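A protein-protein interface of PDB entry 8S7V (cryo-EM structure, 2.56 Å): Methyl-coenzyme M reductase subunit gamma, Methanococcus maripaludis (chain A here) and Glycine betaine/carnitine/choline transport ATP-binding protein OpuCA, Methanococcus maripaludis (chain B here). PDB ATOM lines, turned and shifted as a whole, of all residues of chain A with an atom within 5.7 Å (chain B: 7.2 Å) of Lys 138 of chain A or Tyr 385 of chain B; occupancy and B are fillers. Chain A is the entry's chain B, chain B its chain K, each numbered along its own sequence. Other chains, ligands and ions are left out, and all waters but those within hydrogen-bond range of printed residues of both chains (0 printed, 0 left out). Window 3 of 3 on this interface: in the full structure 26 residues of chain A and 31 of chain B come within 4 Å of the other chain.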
ATOM      1  N   LYS A  30      16.260 -23.875  -4.501  1.00  0.00           N
ATOM      2  CA  LYS A  30      15.884 -23.539  -5.863  1.00  0.00           C
ATOM      3  C   LYS A  30      14.438 -23.063  -5.905  1.00  0.00           C
ATOM      4  O   LYS A  30      13.564 -23.597  -5.218  1.00  0.00           O
ATOM      5  CB  LYS A  30      16.096 -24.733  -6.798  1.00  0.00           C
ATOM      6  CG  LYS A  30      15.093 -25.857  -6.658  1.00  0.00           C
ATOM      7  CD  LYS A  30      15.254 -26.866  -7.784  1.00  0.00           C
ATOM      8  CE  LYS A  30      15.253 -26.187  -9.142  1.00  0.00           C
ATOM      9  NZ  LYS A  30      14.691 -27.061 -10.206  1.00  0.00           N
ATOM     10  N   GLU A  33      12.573 -23.328 -12.448  1.00  0.00           N
ATOM     11  CA  GLU A  33      13.134 -24.332 -13.343  1.00  0.00           C
ATOM     12  C   GLU A  33      13.200 -23.733 -14.740  1.00  0.00           C
ATOM     13  O   GLU A  33      12.182 -23.652 -15.436  1.00  0.00           O
ATOM     14  CB  GLU A  33      12.300 -25.611 -13.330  1.00  0.00           C
ATOM     15  CG  GLU A  33      12.748 -26.654 -14.336  1.00  0.00           C
ATOM     16  CD  GLU A  33      14.067 -27.295 -13.955  1.00  0.00           C
ATOM     17  OE1 GLU A  33      14.352 -27.391 -12.744  1.00  0.00           O
ATOM     18  OE2 GLU A  33      14.819 -27.704 -14.866  1.00  0.00           O
ATOM     19  N   ILE A  34      14.389 -23.309 -15.143  1.00  0.00           N
ATOM     20  CA  ILE A  34      14.647 -22.786 -16.480  1.00  0.00           C
ATOM     21  C   ILE A  34      15.464 -23.831 -17.233  1.00  0.00           C
ATOM     22  O   ILE A  34      16.540 -24.217 -16.761  1.00  0.00           O
ATOM     23  CB  ILE A  34      15.383 -21.438 -16.434  1.00  0.00           C
ATOM     24  CG1 ILE A  34      14.694 -20.487 -15.455  1.00  0.00           C
ATOM     25  CG2 ILE A  34      15.444 -20.818 -17.815  1.00  0.00           C
ATOM     26  CD1 ILE A  34      15.601 -19.412 -14.916  1.00  0.00           C
ATOM     27  N   PRO A  35      14.999 -24.317 -18.380  1.00  0.00           N
ATOM     28  CA  PRO A  35      15.743 -25.355 -19.099  1.00  0.00           C
ATOM     29  C   PRO A  35      17.108 -24.861 -19.550  1.00  0.00           C
ATOM     30  O   PRO A  35      17.345 -23.664 -19.723  1.00  0.00           O
ATOM     31  CB  PRO A  35      14.845 -25.672 -20.300  1.00  0.00           C
ATOM     32  CG  PRO A  35      13.494 -25.168 -19.918  1.00  0.00           C
ATOM     33  CD  PRO A  35      13.731 -23.982 -19.045  1.00  0.00           C
ATOM     34  N   ASP A  36      18.022 -25.820 -19.724  1.00  0.00           N
ATOM     35  CA  ASP A  36      19.387 -25.490 -20.118  1.00  0.00           C
ATOM     36  C   ASP A  36      19.413 -24.706 -21.422  1.00  0.00           C
ATOM     37  O   ASP A  36      20.172 -23.739 -21.559  1.00  0.00           O
ATOM     38  CB  ASP A  36      20.214 -26.770 -20.251  1.00  0.00           C
ATOM     39  CG  ASP A  36      20.917 -27.145 -18.966  1.00  0.00           C
ATOM     40  OD1 ASP A  36      21.734 -26.338 -18.474  1.00  0.00           O
ATOM     41  OD2 ASP A  36      20.656 -28.249 -18.445  1.00  0.00           O
ATOM     42  N   VAL A  39      18.496 -21.083 -20.775  1.00  0.00           N
ATOM     43  CA  VAL A  39      19.620 -20.351 -20.198  1.00  0.00           C
ATOM     44  C   VAL A  39      20.640 -20.019 -21.276  1.00  0.00           C
ATOM     45  O   VAL A  39      21.175 -18.906 -21.323  1.00  0.00           O
ATOM     46  CB  VAL A  39      20.250 -21.160 -19.050  1.00  0.00           C
ATOM     47  CG1 VAL A  39      21.499 -20.467 -18.534  1.00  0.00           C
ATOM     48  CG2 VAL A  39      19.247 -21.360 -17.930  1.00  0.00           C
ATOM     49  N   LEU A 133      30.622 -23.076 -17.797  1.00  0.00           N
ATOM     50  CA  LEU A 133      29.930 -21.829 -17.498  1.00  0.00           C
ATOM     51  C   LEU A 133      28.425 -21.994 -17.629  1.00  0.00           C
ATOM     52  O   LEU A 133      27.671 -21.565 -16.750  1.00  0.00           O
ATOM     53  CB  LEU A 133      30.442 -20.725 -18.420  1.00  0.00           C
ATOM     54  CG  LEU A 133      29.810 -19.340 -18.357  1.00  0.00           C
ATOM     55  CD1 LEU A 133      30.361 -18.566 -17.185  1.00  0.00           C
ATOM     56  CD2 LEU A 133      30.121 -18.618 -19.640  1.00  0.00           C
ATOM     57  N   GLU A 134      27.970 -22.640 -18.702  1.00  0.00           N
ATOM     58  CA  GLU A 134      26.545 -22.914 -18.851  1.00  0.00           C
ATOM     59  C   GLU A 134      26.047 -23.838 -17.748  1.00  0.00           C
ATOM     60  O   GLU A 134      24.952 -23.636 -17.203  1.00  0.00           O
ATOM     61  CB  GLU A 134      26.272 -23.522 -20.225  1.00  0.00           C
ATOM     62  CG  GLU A 134      26.171 -22.501 -21.343  1.00  0.00           C
ATOM     63  CD  GLU A 134      26.430 -23.107 -22.705  1.00  0.00           C
ATOM     64  OE1 GLU A 134      26.398 -24.352 -22.819  1.00  0.00           O
ATOM     65  OE2 GLU A 134      26.664 -22.341 -23.662  1.00  0.00           O
ATOM     66  N   GLU A 135      26.841 -24.854 -17.402  1.00  0.00           N
ATOM     67  CA  GLU A 135      26.427 -25.799 -16.369  1.00  0.00           C
ATOM     68  C   GLU A 135      26.157 -25.093 -15.047  1.00  0.00           C
ATOM     69  O   GLU A 135      25.072 -25.230 -14.467  1.00  0.00           O
ATOM     70  CB  GLU A 135      27.489 -26.881 -16.188  1.00  0.00           C
ATOM     71  CG  GLU A 135      27.394 -27.606 -14.857  1.00  0.00           C
ATOM     72  CD  GLU A 135      28.401 -28.728 -14.725  1.00  0.00           C
ATOM     73  OE1 GLU A 135      29.543 -28.562 -15.201  1.00  0.00           O
ATOM     74  OE2 GLU A 135      28.053 -29.774 -14.139  1.00  0.00           O
ATOM     75  N   PHE A 136      27.122 -24.309 -14.558  1.00  0.00           N
ATOM     76  CA  PHE A 136      26.890 -23.678 -13.263  1.00  0.00           C
ATOM     77  C   PHE A 136      26.035 -22.423 -13.365  1.00  0.00           C
ATOM     78  O   PHE A 136      25.566 -21.934 -12.333  1.00  0.00           O
ATOM     79  CB  PHE A 136      28.210 -23.379 -12.522  1.00  0.00           C
ATOM     80  CG  PHE A 136      29.066 -22.295 -13.133  1.00  0.00           C
ATOM     81  CD1 PHE A 136      28.676 -20.965 -13.111  1.00  0.00           C
ATOM     82  CD2 PHE A 136      30.308 -22.603 -13.653  1.00  0.00           C
ATOM     83  CE1 PHE A 136      29.476 -19.984 -13.652  1.00  0.00           C
ATOM     84  CE2 PHE A 136      31.114 -21.625 -14.191  1.00  0.00           C
ATOM     85  CZ  PHE A 136      30.699 -20.314 -14.188  1.00  0.00           C
ATOM     86  N   SER A 137      25.813 -21.891 -14.568  1.00  0.00           N
ATOM     87  CA  SER A 137      24.838 -20.821 -14.720  1.00  0.00           C
ATOM     88  C   SER A 137      23.425 -21.356 -14.551  1.00  0.00           C
ATOM     89  O   SER A 137      22.587 -20.721 -13.901  1.00  0.00           O
ATOM     90  CB  SER A 137      24.999 -20.156 -16.084  1.00  0.00           C
ATOM     91  OG  SER A 137      26.110 -19.280 -16.094  1.00  0.00           O
ATOM     92  N   LYS A 138      23.141 -22.521 -15.133  1.00  0.00           N
ATOM     93  CA  LYS A 138      21.827 -23.122 -14.943  1.00  0.00           C
ATOM     94  C   LYS A 138      21.655 -23.656 -13.526  1.00  0.00           C
ATOM     95  O   LYS A 138      20.632 -23.401 -12.883  1.00  0.00           O
ATOM     96  CB  LYS A 138      21.604 -24.235 -15.963  1.00  0.00           C
ATOM     97  CG  LYS A 138      20.147 -24.635 -16.125  1.00  0.00           C
ATOM     98  CD  LYS A 138      19.831 -25.885 -15.328  1.00  0.00           C
ATOM     99  CE  LYS A 138      18.480 -26.451 -15.707  1.00  0.00           C
ATOM    100  NZ  LYS A 138      17.383 -25.820 -14.928  1.00  0.00           N
ATOM    101  N   ASN A 139      22.645 -24.394 -13.020  1.00  0.00           N
ATOM    102  CA  ASN A 139      22.466 -25.094 -11.752  1.00  0.00           C
ATOM    103  C   ASN A 139      22.413 -24.157 -10.553  1.00  0.00           C
ATOM    104  O   ASN A 139      21.576 -24.346  -9.665  1.00  0.00           O
ATOM    105  CB  ASN A 139      23.584 -26.115 -11.552  1.00  0.00           C
ATOM    106  CG  ASN A 139      23.328 -27.406 -12.292  1.00  0.00           C
ATOM    107  OD1 ASN A 139      22.260 -27.600 -12.871  1.00  0.00           O
ATOM    108  ND2 ASN A 139      24.308 -28.301 -12.278  1.00  0.00           N
ATOM    109  N   ILE A 140      23.288 -23.154 -10.499  1.00  0.00           N
ATOM    110  CA  ILE A 140      23.467 -22.325  -9.313  1.00  0.00           C
ATOM    111  C   ILE A 140      22.994 -20.896  -9.549  1.00  0.00           C
ATOM    112  O   ILE A 140      22.266 -20.328  -8.731  1.00  0.00           O
ATOM    113  CB  ILE A 140      24.938 -22.340  -8.837  1.00  0.00           C
ATOM    114  CG1 ILE A 140      25.292 -23.702  -8.242  1.00  0.00           C
ATOM    115  CG2 ILE A 140      25.189 -21.235  -7.828  1.00  0.00           C
ATOM    116  CD1 ILE A 140      26.620 -24.243  -8.712  1.00  0.00           C
ATOM    117  N   LEU A 141      23.391 -20.302 -10.672  1.00  0.00           N
ATOM    118  CA  LEU A 141      23.197 -18.869 -10.856  1.00  0.00           C
ATOM    119  C   LEU A 141      21.748 -18.496 -11.141  1.00  0.00           C
ATOM    120  O   LEU A 141      21.307 -17.417 -10.734  1.00  0.00           O
ATOM    121  CB  LEU A 141      24.095 -18.360 -11.983  1.00  0.00           C
ATOM    122  CG  LEU A 141      25.420 -17.720 -11.566  1.00  0.00           C
ATOM    123  CD1 LEU A 141      26.193 -18.626 -10.623  1.00  0.00           C
ATOM    124  CD2 LEU A 141      26.254 -17.386 -12.788  1.00  0.00           C
ATOM    125  N   MET A 142      20.995 -19.353 -11.827  1.00  0.00           N
ATOM    126  CA  MET A 142      19.668 -18.987 -12.310  1.00  0.00           C
ATOM    127  C   MET A 142      18.528 -19.695 -11.598  1.00  0.00           C
ATOM    128  O   MET A 142      17.489 -19.079 -11.355  1.00  0.00           O
ATOM    129  CB  MET A 142      19.562 -19.261 -13.814  1.00  0.00           C
ATOM    130  CG  MET A 142      20.451 -18.375 -14.671  1.00  0.00           C
ATOM    131  SD  MET A 142      19.936 -16.650 -14.691  1.00  0.00           S
ATOM    132  CE  MET A 142      18.289 -16.797 -15.375  1.00  0.00           C
ATOM    133  N   ASP A 143      18.680 -20.971 -11.255  1.00  0.00           N
ATOM    134  CA  ASP A 143      17.583 -21.734 -10.676  1.00  0.00           C
ATOM    135  C   ASP A 143      17.456 -21.581  -9.167  1.00  0.00           C
ATOM    136  O   ASP A 143      16.413 -21.945  -8.617  1.00  0.00           O
ATOM    137  CB  ASP A 143      17.732 -23.221 -11.014  1.00  0.00           C
ATOM    138  CG  ASP A 143      17.340 -23.539 -12.441  1.00  0.00           C
ATOM    139  OD1 ASP A 143      17.139 -22.593 -13.230  1.00  0.00           O
ATOM    140  OD2 ASP A 143      17.230 -24.737 -12.773  1.00  0.00           O
ATOM    141  N   THR A 144      18.467 -21.050  -8.490  1.00  0.00           N
ATOM    142  CA  THR A 144      18.468 -21.023  -7.037  1.00  0.00           C
ATOM    143  C   THR A 144      18.010 -19.656  -6.532  1.00  0.00           C
ATOM    144  O   THR A 144      17.579 -18.792  -7.298  1.00  0.00           O
ATOM    145  CB  THR A 144      19.849 -21.384  -6.499  1.00  0.00           C
ATOM    146  OG1 THR A 144      20.825 -20.496  -7.055  1.00  0.00           O
ATOM    147  CG2 THR A 144      20.203 -22.811  -6.871  1.00  0.00           C
ATOM    148  N   TYR B 378      24.797 -32.119 -23.560  1.00  0.00           N
ATOM    149  CA  TYR B 378      25.307 -31.542 -22.328  1.00  0.00           C
ATOM    150  C   TYR B 378      26.090 -32.613 -21.588  1.00  0.00           C
ATOM    151  O   TYR B 378      25.480 -33.458 -20.917  1.00  0.00           O
ATOM    152  CB  TYR B 378      24.164 -31.010 -21.466  1.00  0.00           C
ATOM    153  CG  TYR B 378      23.343 -29.948 -22.164  1.00  0.00           C
ATOM    154  CD1 TYR B 378      23.697 -28.608 -22.091  1.00  0.00           C
ATOM    155  CD2 TYR B 378      22.225 -30.288 -22.911  1.00  0.00           C
ATOM    156  CE1 TYR B 378      22.954 -27.636 -22.733  1.00  0.00           C
ATOM    157  CE2 TYR B 378      21.476 -29.325 -23.557  1.00  0.00           C
ATOM    158  CZ  TYR B 378      21.844 -28.002 -23.466  1.00  0.00           C
ATOM    159  OH  TYR B 378      21.099 -27.041 -24.110  1.00  0.00           O
ATOM    160  N   HIS B 380      27.703 -32.734 -18.922  1.00  0.00           N
ATOM    161  CA  HIS B 380      27.554 -32.742 -17.475  1.00  0.00           C
ATOM    162  C   HIS B 380      26.271 -33.424 -17.021  1.00  0.00           C
ATOM    163  O   HIS B 380      26.070 -33.591 -15.815  1.00  0.00           O
ATOM    164  CB  HIS B 380      27.591 -31.310 -16.931  1.00  0.00           C
ATOM    165  CG  HIS B 380      26.986 -30.292 -17.850  1.00  0.00           C
ATOM    166  ND1 HIS B 380      25.738 -29.745 -17.634  1.00  0.00           N
ATOM    167  CD2 HIS B 380      27.461 -29.708 -18.974  1.00  0.00           C
ATOM    168  CE1 HIS B 380      25.467 -28.877 -18.593  1.00  0.00           C
ATOM    169  NE2 HIS B 380      26.496 -28.836 -19.419  1.00  0.00           N
ATOM    170  N   ARG B 381      25.408 -33.818 -17.951  1.00  0.00           N
ATOM    171  CA  ARG B 381      24.099 -34.368 -17.645  1.00  0.00           C
ATOM    172  C   ARG B 381      24.022 -35.826 -18.077  1.00  0.00           C
ATOM    173  O   ARG B 381      24.866 -36.322 -18.826  1.00  0.00           O
ATOM    174  CB  ARG B 381      22.997 -33.564 -18.343  1.00  0.00           C
ATOM    175  CG  ARG B 381      23.034 -32.069 -18.070  1.00  0.00           C
ATOM    176  CD  ARG B 381      23.330 -31.763 -16.613  1.00  0.00           C
ATOM    177  NE  ARG B 381      23.082 -30.362 -16.299  1.00  0.00           N
ATOM    178  CZ  ARG B 381      22.581 -29.928 -15.151  1.00  0.00           C
ATOM    179  NH1 ARG B 381      22.272 -30.762 -14.173  1.00  0.00           N
ATOM    180  NH2 ARG B 381      22.386 -28.624 -14.983  1.00  0.00           N
ATOM    181  N   THR B 382      22.996 -36.513 -17.584  1.00  0.00           N
ATOM    182  CA  THR B 382      22.712 -37.864 -18.034  1.00  0.00           C
ATOM    183  C   THR B 382      21.918 -37.829 -19.337  1.00  0.00           C
ATOM    184  O   THR B 382      21.473 -36.775 -19.799  1.00  0.00           O
ATOM    185  CB  THR B 382      21.943 -38.642 -16.967  1.00  0.00           C
ATOM    186  OG1 THR B 382      20.685 -38.004 -16.721  1.00  0.00           O
ATOM    187  CG2 THR B 382      22.736 -38.696 -15.674  1.00  0.00           C
ATOM    188  N   ILE B 383      21.754 -39.006 -19.943  1.00  0.00           N
ATOM    189  CA  ILE B 383      20.961 -39.104 -21.163  1.00  0.00           C
ATOM    190  C   ILE B 383      19.505 -38.750 -20.883  1.00  0.00           C
ATOM    191  O   ILE B 383      18.868 -38.020 -21.656  1.00  0.00           O
ATOM    192  CB  ILE B 383      21.104 -40.509 -21.775  1.00  0.00           C
ATOM    193  CG1 ILE B 383      22.538 -40.736 -22.250  1.00  0.00           C
ATOM    194  CG2 ILE B 383      20.147 -40.694 -22.929  1.00  0.00           C
ATOM    195  CD1 ILE B 383      23.049 -39.652 -23.168  1.00  0.00           C
ATOM    196  N   LEU B 384      18.963 -39.245 -19.769  1.00  0.00           N
ATOM    197  CA  LEU B 384      17.593 -38.912 -19.392  1.00  0.00           C
ATOM    198  C   LEU B 384      17.425 -37.410 -19.207  1.00  0.00           C
ATOM    199  O   LEU B 384      16.441 -36.823 -19.678  1.00  0.00           O
ATOM    200  CB  LEU B 384      17.215 -39.653 -18.111  1.00  0.00           C
ATOM    201  CG  LEU B 384      15.811 -39.435 -17.552  1.00  0.00           C
ATOM    202  CD1 LEU B 384      14.765 -39.702 -18.615  1.00  0.00           C
ATOM    203  CD2 LEU B 384      15.583 -40.316 -16.337  1.00  0.00           C
ATOM    204  N   TYR B 385      18.379 -36.770 -18.529  1.00  0.00           N
ATOM    205  CA  TYR B 385      18.322 -35.324 -18.353  1.00  0.00           C
ATOM    206  C   TYR B 385      18.402 -34.608 -19.695  1.00  0.00           C
ATOM    207  O   TYR B 385      17.713 -33.605 -19.914  1.00  0.00           O
ATOM    208  CB  TYR B 385      19.452 -34.868 -17.431  1.00  0.00           C
ATOM    209  CG  TYR B 385      19.310 -33.450 -16.929  1.00  0.00           C
ATOM    210  CD1 TYR B 385      19.652 -32.371 -17.729  1.00  0.00           C
ATOM    211  CD2 TYR B 385      18.838 -33.194 -15.650  1.00  0.00           C
ATOM    212  CE1 TYR B 385      19.526 -31.077 -17.275  1.00  0.00           C
ATOM    213  CE2 TYR B 385      18.710 -31.902 -15.186  1.00  0.00           C
ATOM    214  CZ  TYR B 385      19.054 -30.849 -16.003  1.00  0.00           C
ATOM    215  OH  TYR B 385      18.927 -29.562 -15.544  1.00  0.00           O
ATOM    216  N   ASN B 386      19.241 -35.109 -20.602  1.00  0.00           N
ATOM    217  CA  ASN B 386      19.362 -34.496 -21.920  1.00  0.00           C
ATOM    218  C   ASN B 386      18.049 -34.571 -22.688  1.00  0.00           C
ATOM    219  O   ASN B 386      17.670 -33.616 -23.374  1.00  0.00           O
ATOM    220  CB  ASN B 386      20.484 -35.169 -22.707  1.00  0.00           C
ATOM    221  CG  ASN B 386      21.815 -34.475 -22.529  1.00  0.00           C
ATOM    222  OD1 ASN B 386      22.073 -33.438 -23.138  1.00  0.00           O
ATOM    223  ND2 ASN B 386      22.671 -35.043 -21.692  1.00  0.00           N
ATOM    224  N   LEU B 387      17.341 -35.699 -22.590  1.00  0.00           N
ATOM    225  CA  LEU B 387      16.069 -35.818 -23.296  1.00  0.00           C
ATOM    226  C   LEU B 387      14.976 -34.977 -22.646  1.00  0.00           C
ATOM    227  O   LEU B 387      14.153 -34.378 -23.348  1.00  0.00           O
ATOM    228  CB  LEU B 387      15.627 -37.279 -23.377  1.00  0.00           C
ATOM    229  CG  LEU B 387      16.120 -38.131 -24.550  1.00  0.00           C
ATOM    230  CD1 LEU B 387      16.501 -37.259 -25.736  1.00  0.00           C
ATOM    231  CD2 LEU B 387      17.264 -39.033 -24.153  1.00  0.00           C
ATOM    232  N   THR B 388      14.941 -34.917 -21.315  1.00  0.00           N
ATOM    233  CA  THR B 388      13.779 -34.384 -20.615  1.00  0.00           C
ATOM    234  C   THR B 388      13.991 -32.980 -20.062  1.00  0.00           C
ATOM    235  O   THR B 388      13.233 -32.067 -20.401  1.00  0.00           O
ATOM    236  CB  THR B 388      13.375 -35.342 -19.488  1.00  0.00           C
ATOM    237  OG1 THR B 388      14.373 -35.322 -18.460  1.00  0.00           O
ATOM    238  CG2 THR B 388      13.236 -36.752 -20.026  1.00  0.00           C
ATOM    239  N   GLU B 389      15.001 -32.773 -19.221  1.00  0.00           N
ATOM    240  CA  GLU B 389      15.119 -31.513 -18.497  1.00  0.00           C
ATOM    241  C   GLU B 389      15.941 -30.461 -19.225  1.00  0.00           C
ATOM    242  O   GLU B 389      15.737 -29.265 -18.987  1.00  0.00           O
ATOM    243  CB  GLU B 389      15.728 -31.755 -17.114  1.00  0.00           C
ATOM    244  CG  GLU B 389      15.154 -32.959 -16.389  1.00  0.00           C
ATOM    245  CD  GLU B 389      15.461 -32.948 -14.906  1.00  0.00           C
ATOM    246  OE1 GLU B 389      15.503 -31.850 -14.315  1.00  0.00           O
ATOM    247  OE2 GLU B 389      15.663 -34.038 -14.331  1.00  0.00           O
ATOM    248  N   SER B 390      16.860 -30.867 -20.102  1.00  0.00           N
ATOM    249  CA  SER B 390      17.735 -29.896 -20.752  1.00  0.00           C
ATOM    250  C   SER B 390      16.973 -29.039 -21.754  1.00  0.00           C
ATOM    251  O   SER B 390      17.323 -27.874 -21.975  1.00  0.00           O
ATOM    252  CB  SER B 390      18.897 -30.615 -21.434  1.00  0.00           C
ATOM    253  OG  SER B 390      20.030 -30.657 -20.585  1.00  0.00           O
ATOM    254  N   ILE B 391      15.901 -29.600 -22.322  1.00  0.00           N
ATOM    255  CA  ILE B 391      15.137 -28.871 -23.380  1.00  0.00           C
ATOM    256  C   ILE B 391      13.754 -28.463 -22.857  1.00  0.00           C
ATOM    257  O   ILE B 391      13.144 -27.569 -23.469  1.00  0.00           O
ATOM    258  CB  ILE B 391      15.025 -29.732 -24.651  1.00  0.00           C
ATOM    259  CG1 ILE B 391      14.390 -31.094 -24.365  1.00  0.00           C
ATOM    260  CG2 ILE B 391      16.381 -29.875 -25.323  1.00  0.00           C
ATOM    261  CD1 ILE B 391      14.417 -32.026 -25.548  1.00  0.00           C
ATOM    262  N   GLY B 392      13.279 -29.094 -21.781  1.00  0.00           N
ATOM    263  CA  GLY B 392      11.983 -28.707 -21.190  1.00  0.00           C
ATOM    264  C   GLY B 392      10.827 -29.486 -21.789  1.00  0.00           C
ATOM    265  O   GLY B 392      10.172 -28.951 -22.702  1.00  0.00           O
ATOM    266  N   ALA B 404      10.979 -40.623 -22.708  1.00  0.00           N
ATOM    267  CA  ALA B 404      12.353 -40.701 -23.193  1.00  0.00           C
ATOM    268  C   ALA B 404      12.695 -42.106 -23.670  1.00  0.00           C
ATOM    269  O   ALA B 404      13.344 -42.273 -24.709  1.00  0.00           O
ATOM    270  CB  ALA B 404      13.323 -40.255 -22.098  1.00  0.00           C
ATOM    271  N   LEU B 422      19.850 -44.738 -20.204  1.00  0.00           N
ATOM    272  CA  LEU B 422      19.218 -43.559 -19.617  1.00  0.00           C
ATOM    273  C   LEU B 422      20.083 -42.933 -18.528  1.00  0.00           C
ATOM    274  O   LEU B 422      20.247 -41.708 -18.486  1.00  0.00           O
ATOM    275  CB  LEU B 422      17.846 -43.933 -19.060  1.00  0.00           C
ATOM    276  CG  LEU B 422      16.682 -43.860 -20.049  1.00  0.00           C
ATOM    277  CD1 LEU B 422      15.357 -43.979 -19.322  1.00  0.00           C
ATOM    278  CD2 LEU B 422      16.740 -42.572 -20.851  1.00  0.00           C
ATOM    279  N   LYS B 424      23.261 -42.657 -18.041  1.00  0.00           N
ATOM    280  CA  LYS B 424      24.623 -42.629 -18.550  1.00  0.00           C
ATOM    281  C   LYS B 424      24.923 -41.235 -19.076  1.00  0.00           C
ATOM    282  O   LYS B 424      24.021 -40.480 -19.444  1.00  0.00           O
ATOM    283  CB  LYS B 424      24.839 -43.674 -19.650  1.00  0.00           C
ATOM    284  CG  LYS B 424      25.103 -45.075 -19.132  1.00  0.00           C
ATOM    285  CD  LYS B 424      25.331 -46.049 -20.275  1.00  0.00           C
ATOM    286  CE  LYS B 424      26.812 -46.290 -20.504  1.00  0.00           C
ATOM    287  NZ  LYS B 424      27.114 -46.537 -21.940  1.00  0.00           N
ATOM    288  N   GLN B 441      16.735 -36.356 -29.223  1.00  0.00           N
ATOM    289  CA  GLN B 441      16.503 -35.064 -28.588  1.00  0.00           C
ATOM    290  C   GLN B 441      15.752 -34.125 -29.520  1.00  0.00           C
ATOM    291  O   GLN B 441      14.870 -33.377 -29.083  1.00  0.00           O
ATOM    292  CB  GLN B 441      17.833 -34.446 -28.161  1.00  0.00           C
ATOM    293  CG  GLN B 441      17.699 -33.216 -27.287  1.00  0.00           C
ATOM    294  CD  GLN B 441      19.020 -32.780 -26.692  1.00  0.00           C
ATOM    295  OE1 GLN B 441      19.851 -33.610 -26.326  1.00  0.00           O
ATOM    296  NE2 GLN B 441      19.223 -31.474 -26.593  1.00  0.00           N
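OD2 of Asp 36 of chain A lies within salt-bridge range of NE of Arg 381 of chain B, 3.9 Å away. O of Ser 390 of chain B is in hydrogen-bond range of N of Asp 36 of chain A, 3.1 Å away. The side-chain amide nitrogen (ND2) of Asn 139 of chain A lies close to the guanidinium group (NH2) of Arg 381 of chain B (3.3 Å).
Pro 35 of chain A touches Glu 389 of chain B. CB of Pro 35 of chain A touches O of Ser 390 of chain B (3.7 Å). CB of Pro 35 of chain A touches C of Ile 391 of chain B, at 3.9 Å. Tyr 378 of chain B touches Asp 36 of chain A (CE1 to CB, 3.8 Å). Tyr 385 of chain B touches Asp 36 of chain A (CE1 to OD2, 3.3 Å). OE2 of Glu 135 of chain A touches CB of His 380 of chain B (3.2 Å). Arg 381 of chain B touches Lys 138 of chain A (NH2 to CD, 3.8 Å). Lys 138 of chain A touches Tyr 385 of chain B.
Of the 18 printed residues of chain A, 5 touch a printed residue of chain B. Printed residues of chain A that touch a printed residue of chain B: Pro 35, Asp 36, Glu 135, Lys 138 and Asn 139. Hydrophobic or aromatic side chains of chain A that line the printed part of chain B: Pro 35. Hydrophobic or aromatic side chains of chain B that line the printed part of chain A: Tyr 378, His 380 and Tyr 385. Among the printed residues, Asp or Glu carboxylates within 4 Å of a Lys or Arg side-chain nitrogen of the other chain: Asp 36 of chain A with Arg 381 of chain B (3.9 Å).
Printed residues of chain B within 4 Å of Lys 138 of chain A: Arg 381 (3.8 Å) and Tyr 385 (3.1 Å). Tyr 385 of chain B touches just these residues of chain A: Asp 36 (3.3 Å) and Lys 138 (3.1 Å). Printed residues of chain B within 4 Å of Asp 36 of chain A: Tyr 378 (3.8 Å), Arg 381 (3.9 Å), Tyr 385 (3.3 Å) and Ser 390 (3.1 Å). Of the printed residues of chain A, His 380 of chain B touches Glu 135. Of the printed residues of chain A, Ile 391 of chain B touches Pro 35. Glu 134 of chain A touches none of the printed residues of chain B. Thr 382 of chain B touches none of the printed residues of chain A. The nearest printed residue of chain A that does not touch Arg 381 of chain B is Glu 135 of chain A (4.4 Å).
OE2 of Glu 33 of chain A lies within salt-bridge range of NZ of Lys 138 of chain A, at 3.2 Å. O of Ile 34 of chain A lies within hydrogen-bond range of NZ of Lys 138 of chain A (2.6 Å). N of Tyr 378 of chain B sits at hydrogen-bond distance from OD1 of Asn 386 of chain B, at 3.1 Å. A ring nitrogen (ND1) of His 380 of chain B lies within hydrogen-bond range of the guanidinium group (NE) of Arg 381 of chain B (3.0 Å). OG1 of Thr 382 of chain B sits at hydrogen-bond distance from N of Tyr 385 of chain B (3.2 Å). The backbone NH (N) of Ser 390 of chain B sits at hydrogen-bond distance from the backbone carbonyl oxygen (O) of Tyr 385 of chain B, 2.9 Å away.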
